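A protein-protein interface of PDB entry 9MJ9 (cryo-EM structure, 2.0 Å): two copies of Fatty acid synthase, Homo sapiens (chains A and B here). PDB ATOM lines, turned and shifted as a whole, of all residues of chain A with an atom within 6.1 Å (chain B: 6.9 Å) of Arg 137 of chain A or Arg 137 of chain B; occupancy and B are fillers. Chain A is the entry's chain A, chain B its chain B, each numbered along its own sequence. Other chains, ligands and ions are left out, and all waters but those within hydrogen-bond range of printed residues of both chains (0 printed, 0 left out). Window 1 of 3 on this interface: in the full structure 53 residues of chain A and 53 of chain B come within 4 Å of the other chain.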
ATOM      1  N   VAL A 111      24.736 -26.191 -16.833  1.00  0.00           N
ATOM      2  CA  VAL A 111      24.769 -25.774 -15.401  1.00  0.00           C
ATOM      3  C   VAL A 111      24.269 -26.962 -14.569  1.00  0.00           C
ATOM      4  O   VAL A 111      23.753 -27.926 -15.173  1.00  0.00           O
ATOM      5  CB  VAL A 111      23.904 -24.524 -15.145  1.00  0.00           C
ATOM      6  CG1 VAL A 111      23.834 -24.163 -13.666  1.00  0.00           C
ATOM      7  CG2 VAL A 111      24.354 -23.330 -15.978  1.00  0.00           C
ATOM      8  N   SER A 112      24.417 -26.894 -13.245  1.00  0.00           N
ATOM      9  CA  SER A 112      23.889 -27.972 -12.370  1.00  0.00           C
ATOM     10  C   SER A 112      23.366 -27.367 -11.063  1.00  0.00           C
ATOM     11  O   SER A 112      22.570 -28.048 -10.381  1.00  0.00           O
ATOM     12  CB  SER A 112      24.934 -29.023 -12.100  1.00  0.00           C
ATOM     13  OG  SER A 112      26.026 -28.476 -11.374  1.00  0.00           O
ATOM     14  N   GLY A 113      23.790 -26.143 -10.726  1.00  0.00           N
ATOM     15  CA  GLY A 113      23.371 -25.594  -9.449  1.00  0.00           C
ATOM     16  C   GLY A 113      23.099 -24.116  -9.547  1.00  0.00           C
ATOM     17  O   GLY A 113      23.691 -23.408 -10.364  1.00  0.00           O
ATOM     18  N   SER A 114      22.176 -23.648  -8.710  1.00  0.00           N
ATOM     19  CA  SER A 114      21.904 -22.223  -8.544  1.00  0.00           C
ATOM     20  C   SER A 114      21.768 -21.962  -7.049  1.00  0.00           C
ATOM     21  O   SER A 114      20.662 -21.968  -6.507  1.00  0.00           O
ATOM     22  CB  SER A 114      20.657 -21.813  -9.312  1.00  0.00           C
ATOM     23  OG  SER A 114      19.549 -22.606  -8.933  1.00  0.00           O
ATOM     24  N   CYS A 135      19.492 -14.647 -11.675  1.00  0.00           N
ATOM     25  CA  CYS A 135      19.878 -15.908 -11.054  1.00  0.00           C
ATOM     26  C   CYS A 135      19.093 -17.126 -11.514  1.00  0.00           C
ATOM     27  O   CYS A 135      19.448 -18.238 -11.112  1.00  0.00           O
ATOM     28  CB  CYS A 135      19.759 -15.815  -9.526  1.00  0.00           C
ATOM     29  SG  CYS A 135      20.980 -14.768  -8.730  1.00  0.00           S
ATOM     30  N   GLN A 136      18.040 -16.964 -12.308  1.00  0.00           N
ATOM     31  CA  GLN A 136      17.310 -18.105 -12.846  1.00  0.00           C
ATOM     32  C   GLN A 136      18.187 -18.859 -13.841  1.00  0.00           C
ATOM     33  O   GLN A 136      18.978 -18.254 -14.563  1.00  0.00           O
ATOM     34  CB  GLN A 136      16.008 -17.613 -13.488  1.00  0.00           C
ATOM     35  CG  GLN A 136      15.391 -18.479 -14.565  1.00  0.00           C
ATOM     36  CD  GLN A 136      14.362 -19.437 -14.024  1.00  0.00           C
ATOM     37  OE1 GLN A 136      14.301 -19.685 -12.822  1.00  0.00           O
ATOM     38  NE2 GLN A 136      13.555 -19.999 -14.910  1.00  0.00           N
ATOM     39  N   ARG A 137      18.070 -20.193 -13.842  1.00  0.00           N
ATOM     40  CA  ARG A 137      18.992 -21.040 -14.596  1.00  0.00           C
ATOM     41  C   ARG A 137      18.870 -20.855 -16.106  1.00  0.00           C
ATOM     42  O   ARG A 137      19.857 -21.037 -16.822  1.00  0.00           O
ATOM     43  CB  ARG A 137      18.775 -22.505 -14.232  1.00  0.00           C
ATOM     44  CG  ARG A 137      19.989 -23.360 -14.489  1.00  0.00           C
ATOM     45  CD  ARG A 137      19.808 -24.777 -14.018  1.00  0.00           C
ATOM     46  NE  ARG A 137      19.760 -24.886 -12.568  1.00  0.00           N
ATOM     47  CZ  ARG A 137      19.856 -26.030 -11.913  1.00  0.00           C
ATOM     48  NH1 ARG A 137      20.047 -27.175 -12.545  1.00  0.00           N
ATOM     49  NH2 ARG A 137      19.753 -26.030 -10.587  1.00  0.00           N
ATOM     50  N   ALA A 138      17.694 -20.484 -16.610  1.00  0.00           N
ATOM     51  CA  ALA A 138      17.559 -20.221 -18.041  1.00  0.00           C
ATOM     52  C   ALA A 138      18.244 -18.924 -18.439  1.00  0.00           C
ATOM     53  O   ALA A 138      18.607 -18.733 -19.609  1.00  0.00           O
ATOM     54  CB  ALA A 138      16.086 -20.170 -18.430  1.00  0.00           C
ATOM     55  N   MET A 139      18.446 -18.027 -17.481  1.00  0.00           N
ATOM     56  CA  MET A 139      19.029 -16.741 -17.805  1.00  0.00           C
ATOM     57  C   MET A 139      20.524 -16.844 -18.055  1.00  0.00           C
ATOM     58  O   MET A 139      21.078 -15.950 -18.692  1.00  0.00           O
ATOM     59  CB  MET A 139      18.723 -15.747 -16.688  1.00  0.00           C
ATOM     60  CG  MET A 139      17.225 -15.520 -16.464  1.00  0.00           C
ATOM     61  SD  MET A 139      16.145 -14.605 -17.598  1.00  0.00           S
ATOM     62  CE  MET A 139      17.248 -13.696 -18.663  1.00  0.00           C
ATOM     63  N   MET A 140      21.159 -17.949 -17.642  1.00  0.00           N
ATOM     64  CA  MET A 140      22.571 -18.186 -17.933  1.00  0.00           C
ATOM     65  C   MET A 140      22.839 -18.303 -19.426  1.00  0.00           C
ATOM     66  O   MET A 140      23.951 -18.016 -19.875  1.00  0.00           O
ATOM     67  CB  MET A 140      23.056 -19.454 -17.230  1.00  0.00           C
ATOM     68  CG  MET A 140      22.702 -19.555 -15.762  1.00  0.00           C
ATOM     69  SD  MET A 140      23.735 -18.550 -14.692  1.00  0.00           S
ATOM     70  CE  MET A 140      22.517 -17.421 -14.039  1.00  0.00           C
ATOM     71  N   ALA A 141      21.850 -18.722 -20.209  1.00  0.00           N
ATOM     72  CA  ALA A 141      21.939 -18.666 -21.659  1.00  0.00           C
ATOM     73  C   ALA A 141      21.203 -17.474 -22.253  1.00  0.00           C
ATOM     74  O   ALA A 141      21.660 -16.914 -23.263  1.00  0.00           O
ATOM     75  CB  ALA A 141      21.387 -19.953 -22.271  1.00  0.00           C
ATOM     76  N   ALA A 156      19.643 -23.854 -21.553  1.00  0.00           N
ATOM     77  CA  ALA A 156      20.440 -24.297 -20.419  1.00  0.00           C
ATOM     78  C   ALA A 156      20.023 -25.711 -20.048  1.00  0.00           C
ATOM     79  O   ALA A 156      18.838 -25.968 -19.829  1.00  0.00           O
ATOM     80  CB  ALA A 156      20.261 -23.367 -19.223  1.00  0.00           C
ATOM     81  N   ASP A 158      20.918 -29.563 -17.894  1.00  0.00           N
ATOM     82  CA  ASP A 158      21.563 -30.217 -16.765  1.00  0.00           C
ATOM     83  C   ASP A 158      21.517 -31.722 -16.963  1.00  0.00           C
ATOM     84  O   ASP A 158      20.434 -32.302 -17.067  1.00  0.00           O
ATOM     85  CB  ASP A 158      20.885 -29.842 -15.450  1.00  0.00           C
ATOM     86  CG  ASP A 158      21.537 -30.502 -14.253  1.00  0.00           C
ATOM     87  OD1 ASP A 158      22.768 -30.688 -14.270  1.00  0.00           O
ATOM     88  OD2 ASP A 158      20.823 -30.821 -13.286  1.00  0.00           O
ATOM     89  N   VAL B 109      12.850 -33.639 -20.514  1.00  0.00           N
ATOM     90  CA  VAL B 109      11.960 -33.105 -19.486  1.00  0.00           C
ATOM     91  C   VAL B 109      12.233 -31.618 -19.328  1.00  0.00           C
ATOM     92  O   VAL B 109      13.392 -31.204 -19.229  1.00  0.00           O
ATOM     93  CB  VAL B 109      12.139 -33.834 -18.139  1.00  0.00           C
ATOM     94  CG1 VAL B 109      11.112 -33.374 -17.139  1.00  0.00           C
ATOM     95  CG2 VAL B 109      12.020 -35.325 -18.320  1.00  0.00           C
ATOM     96  N   VAL B 111      12.001 -28.738 -16.806  1.00  0.00           N
ATOM     97  CA  VAL B 111      11.808 -28.352 -15.378  1.00  0.00           C
ATOM     98  C   VAL B 111      12.254 -26.891 -15.237  1.00  0.00           C
ATOM     99  O   VAL B 111      12.856 -26.366 -16.197  1.00  0.00           O
ATOM    100  CB  VAL B 111      12.605 -29.261 -14.423  1.00  0.00           C
ATOM    101  CG1 VAL B 111      12.512 -28.800 -12.974  1.00  0.00           C
ATOM    102  CG2 VAL B 111      12.211 -30.727 -14.557  1.00  0.00           C
ATOM    103  N   SER B 112      11.967 -26.266 -14.094  1.00  0.00           N
ATOM    104  CA  SER B 112      12.432 -24.876 -13.857  1.00  0.00           C
ATOM    105  C   SER B 112      12.800 -24.698 -12.380  1.00  0.00           C
ATOM    106  O   SER B 112      13.540 -23.739 -12.072  1.00  0.00           O
ATOM    107  CB  SER B 112      11.396 -23.868 -14.282  1.00  0.00           C
ATOM    108  OG  SER B 112      10.219 -23.990 -13.494  1.00  0.00           O
ATOM    109  N   GLY B 113      12.308 -25.580 -11.502  1.00  0.00           N
ATOM    110  CA  GLY B 113      12.576 -25.375 -10.090  1.00  0.00           C
ATOM    111  C   GLY B 113      12.815 -26.680  -9.379  1.00  0.00           C
ATOM    112  O   GLY B 113      12.290 -27.726  -9.765  1.00  0.00           O
ATOM    113  N   SER B 114      13.632 -26.619  -8.329  1.00  0.00           N
ATOM    114  CA  SER B 114      13.845 -27.741  -7.421  1.00  0.00           C
ATOM    115  C   SER B 114      13.817 -27.185  -6.003  1.00  0.00           C
ATOM    116  O   SER B 114      14.861 -26.865  -5.432  1.00  0.00           O
ATOM    117  CB  SER B 114      15.152 -28.454  -7.731  1.00  0.00           C
ATOM    118  OG  SER B 114      16.237 -27.548  -7.707  1.00  0.00           O
ATOM    119  N   GLU B 115      12.620 -27.072  -5.441  1.00  0.00           N
ATOM    120  CA  GLU B 115      12.454 -26.589  -4.081  1.00  0.00           C
ATOM    121  C   GLU B 115      12.565 -27.695  -3.047  1.00  0.00           C
ATOM    122  O   GLU B 115      12.981 -27.427  -1.913  1.00  0.00           O
ATOM    123  CB  GLU B 115      11.103 -25.886  -3.945  1.00  0.00           C
ATOM    124  CG  GLU B 115      10.992 -24.610  -4.756  1.00  0.00           C
ATOM    125  CD  GLU B 115       9.607 -24.397  -5.339  1.00  0.00           C
ATOM    126  OE1 GLU B 115       8.762 -25.302  -5.222  1.00  0.00           O
ATOM    127  OE2 GLU B 115       9.360 -23.320  -5.917  1.00  0.00           O
ATOM    128  N   SER B 117      14.727 -30.045  -3.205  1.00  0.00           N
ATOM    129  CA  SER B 117      16.158 -30.222  -3.009  1.00  0.00           C
ATOM    130  C   SER B 117      16.696 -29.290  -1.938  1.00  0.00           C
ATOM    131  O   SER B 117      17.520 -29.695  -1.113  1.00  0.00           O
ATOM    132  CB  SER B 117      16.892 -29.995  -4.327  1.00  0.00           C
ATOM    133  OG  SER B 117      18.289 -29.999  -4.123  1.00  0.00           O
ATOM    134  N   MET B 132      20.167 -36.416  -2.713  1.00  0.00           N
ATOM    135  CA  MET B 132      20.844 -36.035  -3.943  1.00  0.00           C
ATOM    136  C   MET B 132      20.312 -36.839  -5.122  1.00  0.00           C
ATOM    137  O   MET B 132      20.102 -36.294  -6.208  1.00  0.00           O
ATOM    138  CB  MET B 132      22.348 -36.239  -3.791  1.00  0.00           C
ATOM    139  CG  MET B 132      23.174 -35.760  -4.960  1.00  0.00           C
ATOM    140  SD  MET B 132      23.659 -34.040  -4.760  1.00  0.00           S
ATOM    141  CE  MET B 132      22.687 -33.259  -6.035  1.00  0.00           C
ATOM    142  N   CYS B 135      16.350 -35.767  -5.895  1.00  0.00           N
ATOM    143  CA  CYS B 135      15.937 -34.379  -6.062  1.00  0.00           C
ATOM    144  C   CYS B 135      16.801 -33.554  -7.004  1.00  0.00           C
ATOM    145  O   CYS B 135      16.438 -32.407  -7.277  1.00  0.00           O
ATOM    146  CB  CYS B 135      15.895 -33.663  -4.706  1.00  0.00           C
ATOM    147  SG  CYS B 135      14.568 -34.179  -3.614  1.00  0.00           S
ATOM    148  N   GLN B 136      17.926 -34.074  -7.485  1.00  0.00           N
ATOM    149  CA  GLN B 136      18.739 -33.358  -8.458  1.00  0.00           C
ATOM    150  C   GLN B 136      17.992 -33.256  -9.785  1.00  0.00           C
ATOM    151  O   GLN B 136      17.264 -34.170 -10.165  1.00  0.00           O
ATOM    152  CB  GLN B 136      20.087 -34.072  -8.613  1.00  0.00           C
ATOM    153  CG  GLN B 136      20.837 -33.874  -9.912  1.00  0.00           C
ATOM    154  CD  GLN B 136      21.831 -32.744  -9.844  1.00  0.00           C
ATOM    155  OE1 GLN B 136      21.773 -31.907  -8.947  1.00  0.00           O
ATOM    156  NE2 GLN B 136      22.742 -32.700 -10.805  1.00  0.00           N
ATOM    157  N   ARG B 137      18.148 -32.112 -10.466  1.00  0.00           N
ATOM    158  CA  ARG B 137      17.334 -31.808 -11.641  1.00  0.00           C
ATOM    159  C   ARG B 137      17.605 -32.746 -12.814  1.00  0.00           C
ATOM    160  O   ARG B 137      16.703 -32.991 -13.617  1.00  0.00           O
ATOM    161  CB  ARG B 137      17.553 -30.361 -12.071  1.00  0.00           C
ATOM    162  CG  ARG B 137      16.397 -29.800 -12.857  1.00  0.00           C
ATOM    163  CD  ARG B 137      16.569 -28.340 -13.174  1.00  0.00           C
ATOM    164  NE  ARG B 137      16.469 -27.493 -11.996  1.00  0.00           N
ATOM    165  CZ  ARG B 137      16.339 -26.177 -12.044  1.00  0.00           C
ATOM    166  NH1 ARG B 137      16.248 -25.533 -13.195  1.00  0.00           N
ATOM    167  NH2 ARG B 137      16.304 -25.486 -10.908  1.00  0.00           N
ATOM    168  N   ALA B 138      18.816 -33.290 -12.927  1.00  0.00           N
ATOM    169  CA  ALA B 138      19.090 -34.254 -13.990  1.00  0.00           C
ATOM    170  C   ALA B 138      18.414 -35.588 -13.725  1.00  0.00           C
ATOM    171  O   ALA B 138      18.169 -36.369 -14.657  1.00  0.00           O
ATOM    172  CB  ALA B 138      20.594 -34.455 -14.141  1.00  0.00           C
ATOM    173  N   MET B 139      18.088 -35.863 -12.468  1.00  0.00           N
ATOM    174  CA  MET B 139      17.505 -37.146 -12.135  1.00  0.00           C
ATOM    175  C   MET B 139      16.048 -37.233 -12.556  1.00  0.00           C
ATOM    176  O   MET B 139      15.538 -38.343 -12.689  1.00  0.00           O
ATOM    177  CB  MET B 139      17.664 -37.408 -10.640  1.00  0.00           C
ATOM    178  CG  MET B 139      19.125 -37.441 -10.177  1.00  0.00           C
ATOM    179  SD  MET B 139      20.289 -38.779 -10.553  1.00  0.00           S
ATOM    180  CE  MET B 139      19.278 -40.140 -11.099  1.00  0.00           C
ATOM    181  N   MET B 140      15.405 -36.092 -12.844  1.00  0.00           N
ATOM    182  CA  MET B 140      14.038 -36.083 -13.360  1.00  0.00           C
ATOM    183  C   MET B 140      13.931 -36.767 -14.716  1.00  0.00           C
ATOM    184  O   MET B 140      12.862 -37.277 -15.062  1.00  0.00           O
ATOM    185  CB  MET B 140      13.519 -34.650 -13.472  1.00  0.00           C
ATOM    186  CG  MET B 140      13.722 -33.791 -12.243  1.00  0.00           C
ATOM    187  SD  MET B 140      12.556 -34.124 -10.920  1.00  0.00           S
ATOM    188  CE  MET B 140      13.667 -34.715  -9.653  1.00  0.00           C
ATOM    189  N   ALA B 141      15.006 -36.785 -15.496  1.00  0.00           N
ATOM    190  CA  ALA B 141      15.067 -37.588 -16.705  1.00  0.00           C
ATOM    191  C   ALA B 141      15.825 -38.893 -16.515  1.00  0.00           C
ATOM    192  O   ALA B 141      15.460 -39.909 -17.128  1.00  0.00           O
ATOM    193  CB  ALA B 141      15.715 -36.791 -17.836  1.00  0.00           C
ATOM    194  N   ASN B 142      16.855 -38.892 -15.667  1.00  0.00           N
ATOM    195  CA  ASN B 142      17.687 -40.082 -15.530  1.00  0.00           C
ATOM    196  C   ASN B 142      16.971 -41.219 -14.806  1.00  0.00           C
ATOM    197  O   ASN B 142      17.215 -42.383 -15.126  1.00  0.00           O
ATOM    198  CB  ASN B 142      18.991 -39.729 -14.829  1.00  0.00           C
ATOM    199  CG  ASN B 142      19.948 -38.983 -15.728  1.00  0.00           C
ATOM    200  OD1 ASN B 142      19.911 -39.123 -16.944  1.00  0.00           O
ATOM    201  ND2 ASN B 142      20.821 -38.191 -15.133  1.00  0.00           N
ATOM    202  N   ILE B 155      17.908 -35.878 -21.102  1.00  0.00           N
ATOM    203  CA  ILE B 155      18.246 -34.479 -20.867  1.00  0.00           C
ATOM    204  C   ILE B 155      17.126 -33.791 -20.103  1.00  0.00           C
ATOM    205  O   ILE B 155      15.947 -33.944 -20.439  1.00  0.00           O
ATOM    206  CB  ILE B 155      18.520 -33.741 -22.199  1.00  0.00           C
ATOM    207  CG1 ILE B 155      19.549 -34.486 -23.041  1.00  0.00           C
ATOM    208  CG2 ILE B 155      18.985 -32.326 -21.966  1.00  0.00           C
ATOM    209  CD1 ILE B 155      19.651 -33.999 -24.443  1.00  0.00           C
ATOM    210  N   ALA B 156      17.487 -33.034 -19.071  1.00  0.00           N
ATOM    211  CA  ALA B 156      16.590 -32.091 -18.421  1.00  0.00           C
ATOM    212  C   ALA B 156      17.006 -30.678 -18.798  1.00  0.00           C
ATOM    213  O   ALA B 156      18.169 -30.310 -18.623  1.00  0.00           O
ATOM    214  CB  ALA B 156      16.617 -32.260 -16.906  1.00  0.00           C
ATOM    215  N   LEU B 157      16.067 -29.882 -19.306  1.00  0.00           N
ATOM    216  CA  LEU B 157      16.411 -28.561 -19.810  1.00  0.00           C
ATOM    217  C   LEU B 157      15.479 -27.508 -19.236  1.00  0.00           C
ATOM    218  O   LEU B 157      14.316 -27.785 -18.950  1.00  0.00           O
ATOM    219  CB  LEU B 157      16.386 -28.533 -21.341  1.00  0.00           C
ATOM    220  CG  LEU B 157      15.142 -28.951 -22.116  1.00  0.00           C
ATOM    221  CD1 LEU B 157      14.318 -27.754 -22.514  1.00  0.00           C
ATOM    222  CD2 LEU B 157      15.549 -29.731 -23.337  1.00  0.00           C
ATOM    223  N   ASP B 158      16.005 -26.295 -19.062  1.00  0.00           N
ATOM    224  CA  ASP B 158      15.264 -25.170 -18.510  1.00  0.00           C
ATOM    225  C   ASP B 158      15.374 -23.985 -19.455  1.00  0.00           C
ATOM    226  O   ASP B 158      16.478 -23.512 -19.732  1.00  0.00           O
ATOM    227  CB  ASP B 158      15.792 -24.787 -17.130  1.00  0.00           C
ATOM    228  CG  ASP B 158      15.039 -23.622 -16.525  1.00  0.00           C
ATOM    229  OD1 ASP B 158      13.822 -23.508 -16.763  1.00  0.00           O
ATOM    230  OD2 ASP B 158      15.658 -22.827 -15.796  1.00  0.00           O
ATOM    231  N   THR B 159      14.237 -23.514 -19.949  1.00  0.00           N
ATOM    232  CA  THR B 159      14.207 -22.452 -20.950  1.00  0.00           C
ATOM    233  C   THR B 159      13.051 -21.507 -20.566  1.00  0.00           C
ATOM    234  O   THR B 159      12.338 -20.948 -21.400  1.00  0.00           O
ATOM    235  CB  THR B 159      14.115 -23.122 -22.333  1.00  0.00           C
ATOM    236  OG1 THR B 159      15.257 -23.963 -22.507  1.00  0.00           O
ATOM    237  CG2 THR B 159      14.301 -22.167 -23.460  1.00  0.00           C
ATOM    238  N   ALA B 160      12.867 -21.340 -19.259  1.00  0.00           N
ATOM    239  CA  ALA B 160      11.807 -20.544 -18.585  1.00  0.00           C
ATOM    240  C   ALA B 160      10.445 -21.104 -19.004  1.00  0.00           C
ATOM    241  O   ALA B 160      10.222 -22.317 -18.894  1.00  0.00           O
ATOM    242  CB  ALA B 160      11.997 -19.063 -18.836  1.00  0.00           C
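The backbone NH (N) of Ala 138 of chain A sits at hydrogen-bond distance from the side-chain carboxylate (OD2) of Asp 158 of chain B, 3.2 Å away.
The backbone carbonyl oxygen of Ala 156 of chain A is in hydrogen-bond range of the backbone NH of Asp 158 of chain B (3.0 Å).
The side-chain carboxylate (OD2) of Asp 158 of chain A lies within hydrogen-bond range of the backbone NH (N) of Ala 138 of chain B (3.2 Å).
The backbone carbonyl oxygen (O) of Ala 156 of chain B is in hydrogen-bond range of the backbone NH (N) of Asp 158 of chain A.
The backbone carbonyl oxygen of Ser 112 of chain A lies within hydrogen-bond range of the guanidinium group of Arg 137 of chain A, 3.4 Å away.
NH1 of Arg 137 of chain A is in salt-bridge range of OD2 of Asp 158 of chain A, at 3.8 Å.
O of Leu 157 of chain B sits at hydrogen-bond distance from N of Val 111 of chain B (3.3 Å).
The backbone carbonyl oxygen (O) of Ser 112 of chain B is in hydrogen-bond range of the guanidinium group (NH1) of Arg 137 of chain B (3.4 Å).
O of Ala 138 of chain B sits at hydrogen-bond distance from ND2 of Asn 142 of chain B, 3.3 Å away.
The backbone NH of Ala 160 of chain B lies within hydrogen-bond range of the side-chain carboxylate of Asp 158 of chain B, at 3.4 Å.
Gln 136 of chain A touches Asp 158 of chain B.
Arg 137 of chain A touches Arg 137 of chain B (NH2 to NH2, 3.5 Å).
CB of Arg 137 of chain A touches OD2 of Asp 158 of chain B, at 3.5 Å.
Ala 138 of chain A touches Thr 159 of chain B.
Ala 160 of chain B touches Ala 138 of chain A (N to CB, 3.5 Å).
Ala 156 of chain A touches Leu 157 of chain B (O to CA, 3.6 Å).
NE2 of Gln 136 of chain B touches OD2 of Asp 158 of chain A, 3.7 Å away.
Asp 158 of chain A touches Arg 137 of chain B (OD2 to CB, 3.5 Å).
Printed residues of chain A within 4 Å of Arg 137 of chain B: Arg 137 (3.5 Å) and Asp 158 (3.5 Å).
Of the printed residues of chain B, Gln 136 of chain A touches Asp 158.
Of the printed residues of chain B, Ala 138 of chain A touches Asp 158, Thr 159 and Ala 160.
Of the printed residues of chain A, Ala 156 of chain B touches Asp 158 (2.9 Å).
Of the printed residues of chain B, Asp 158 of chain A touches Gln 136, Arg 137, Ala 138 and Ala 156.
Printed residues of chain A within 4 Å of Leu 157 of chain B: Ala 156 (3.6 Å).
Met 139 of chain B touches none of the printed residues of chain A.
Ser 112 of chain A touches none of the printed residues of chain B.
The nearest residue of chain B that does not touch Arg 137 of chain A is Ser 114 of chain B (4.8 Å).
Along chain A the printed residues that touch a printed residue of chain B span positions 136 to 158.
Of the 22 printed residues of chain B, 8 touch a printed residue of chain A.
Printed residues of chain B that touch a printed residue of chain A: Gln 136, Arg 137, Ala 138, Ala 156, Leu 157, Asp 158, Thr 159 and Ala 160.
Among the printed residues, 12 pairs touch across the chains.
Gln 136 of chain A touches Asp 158 of chain B, and with the chains exchanged Asp 158 of chain A touches Gln 136 of chain B.
Arg 137 of chain A touches Asp 158 of chain B, and with the chains exchanged Asp 158 of chain A touches Arg 137 of chain B.
Ala 138 of chain A touches Asp 158 of chain B, and with the chains exchanged Asp 158 of chain A touches Ala 138 of chain B.
Ala 156 of chain A touches Asp 158 of chain B, and with the chains exchanged Asp 158 of chain A touches Ala 156 of chain B.
Positions printed for both chains: 111, 112, 113, 114, 135, 136, 137, 138, 139, 140, 141, 156 and 158.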
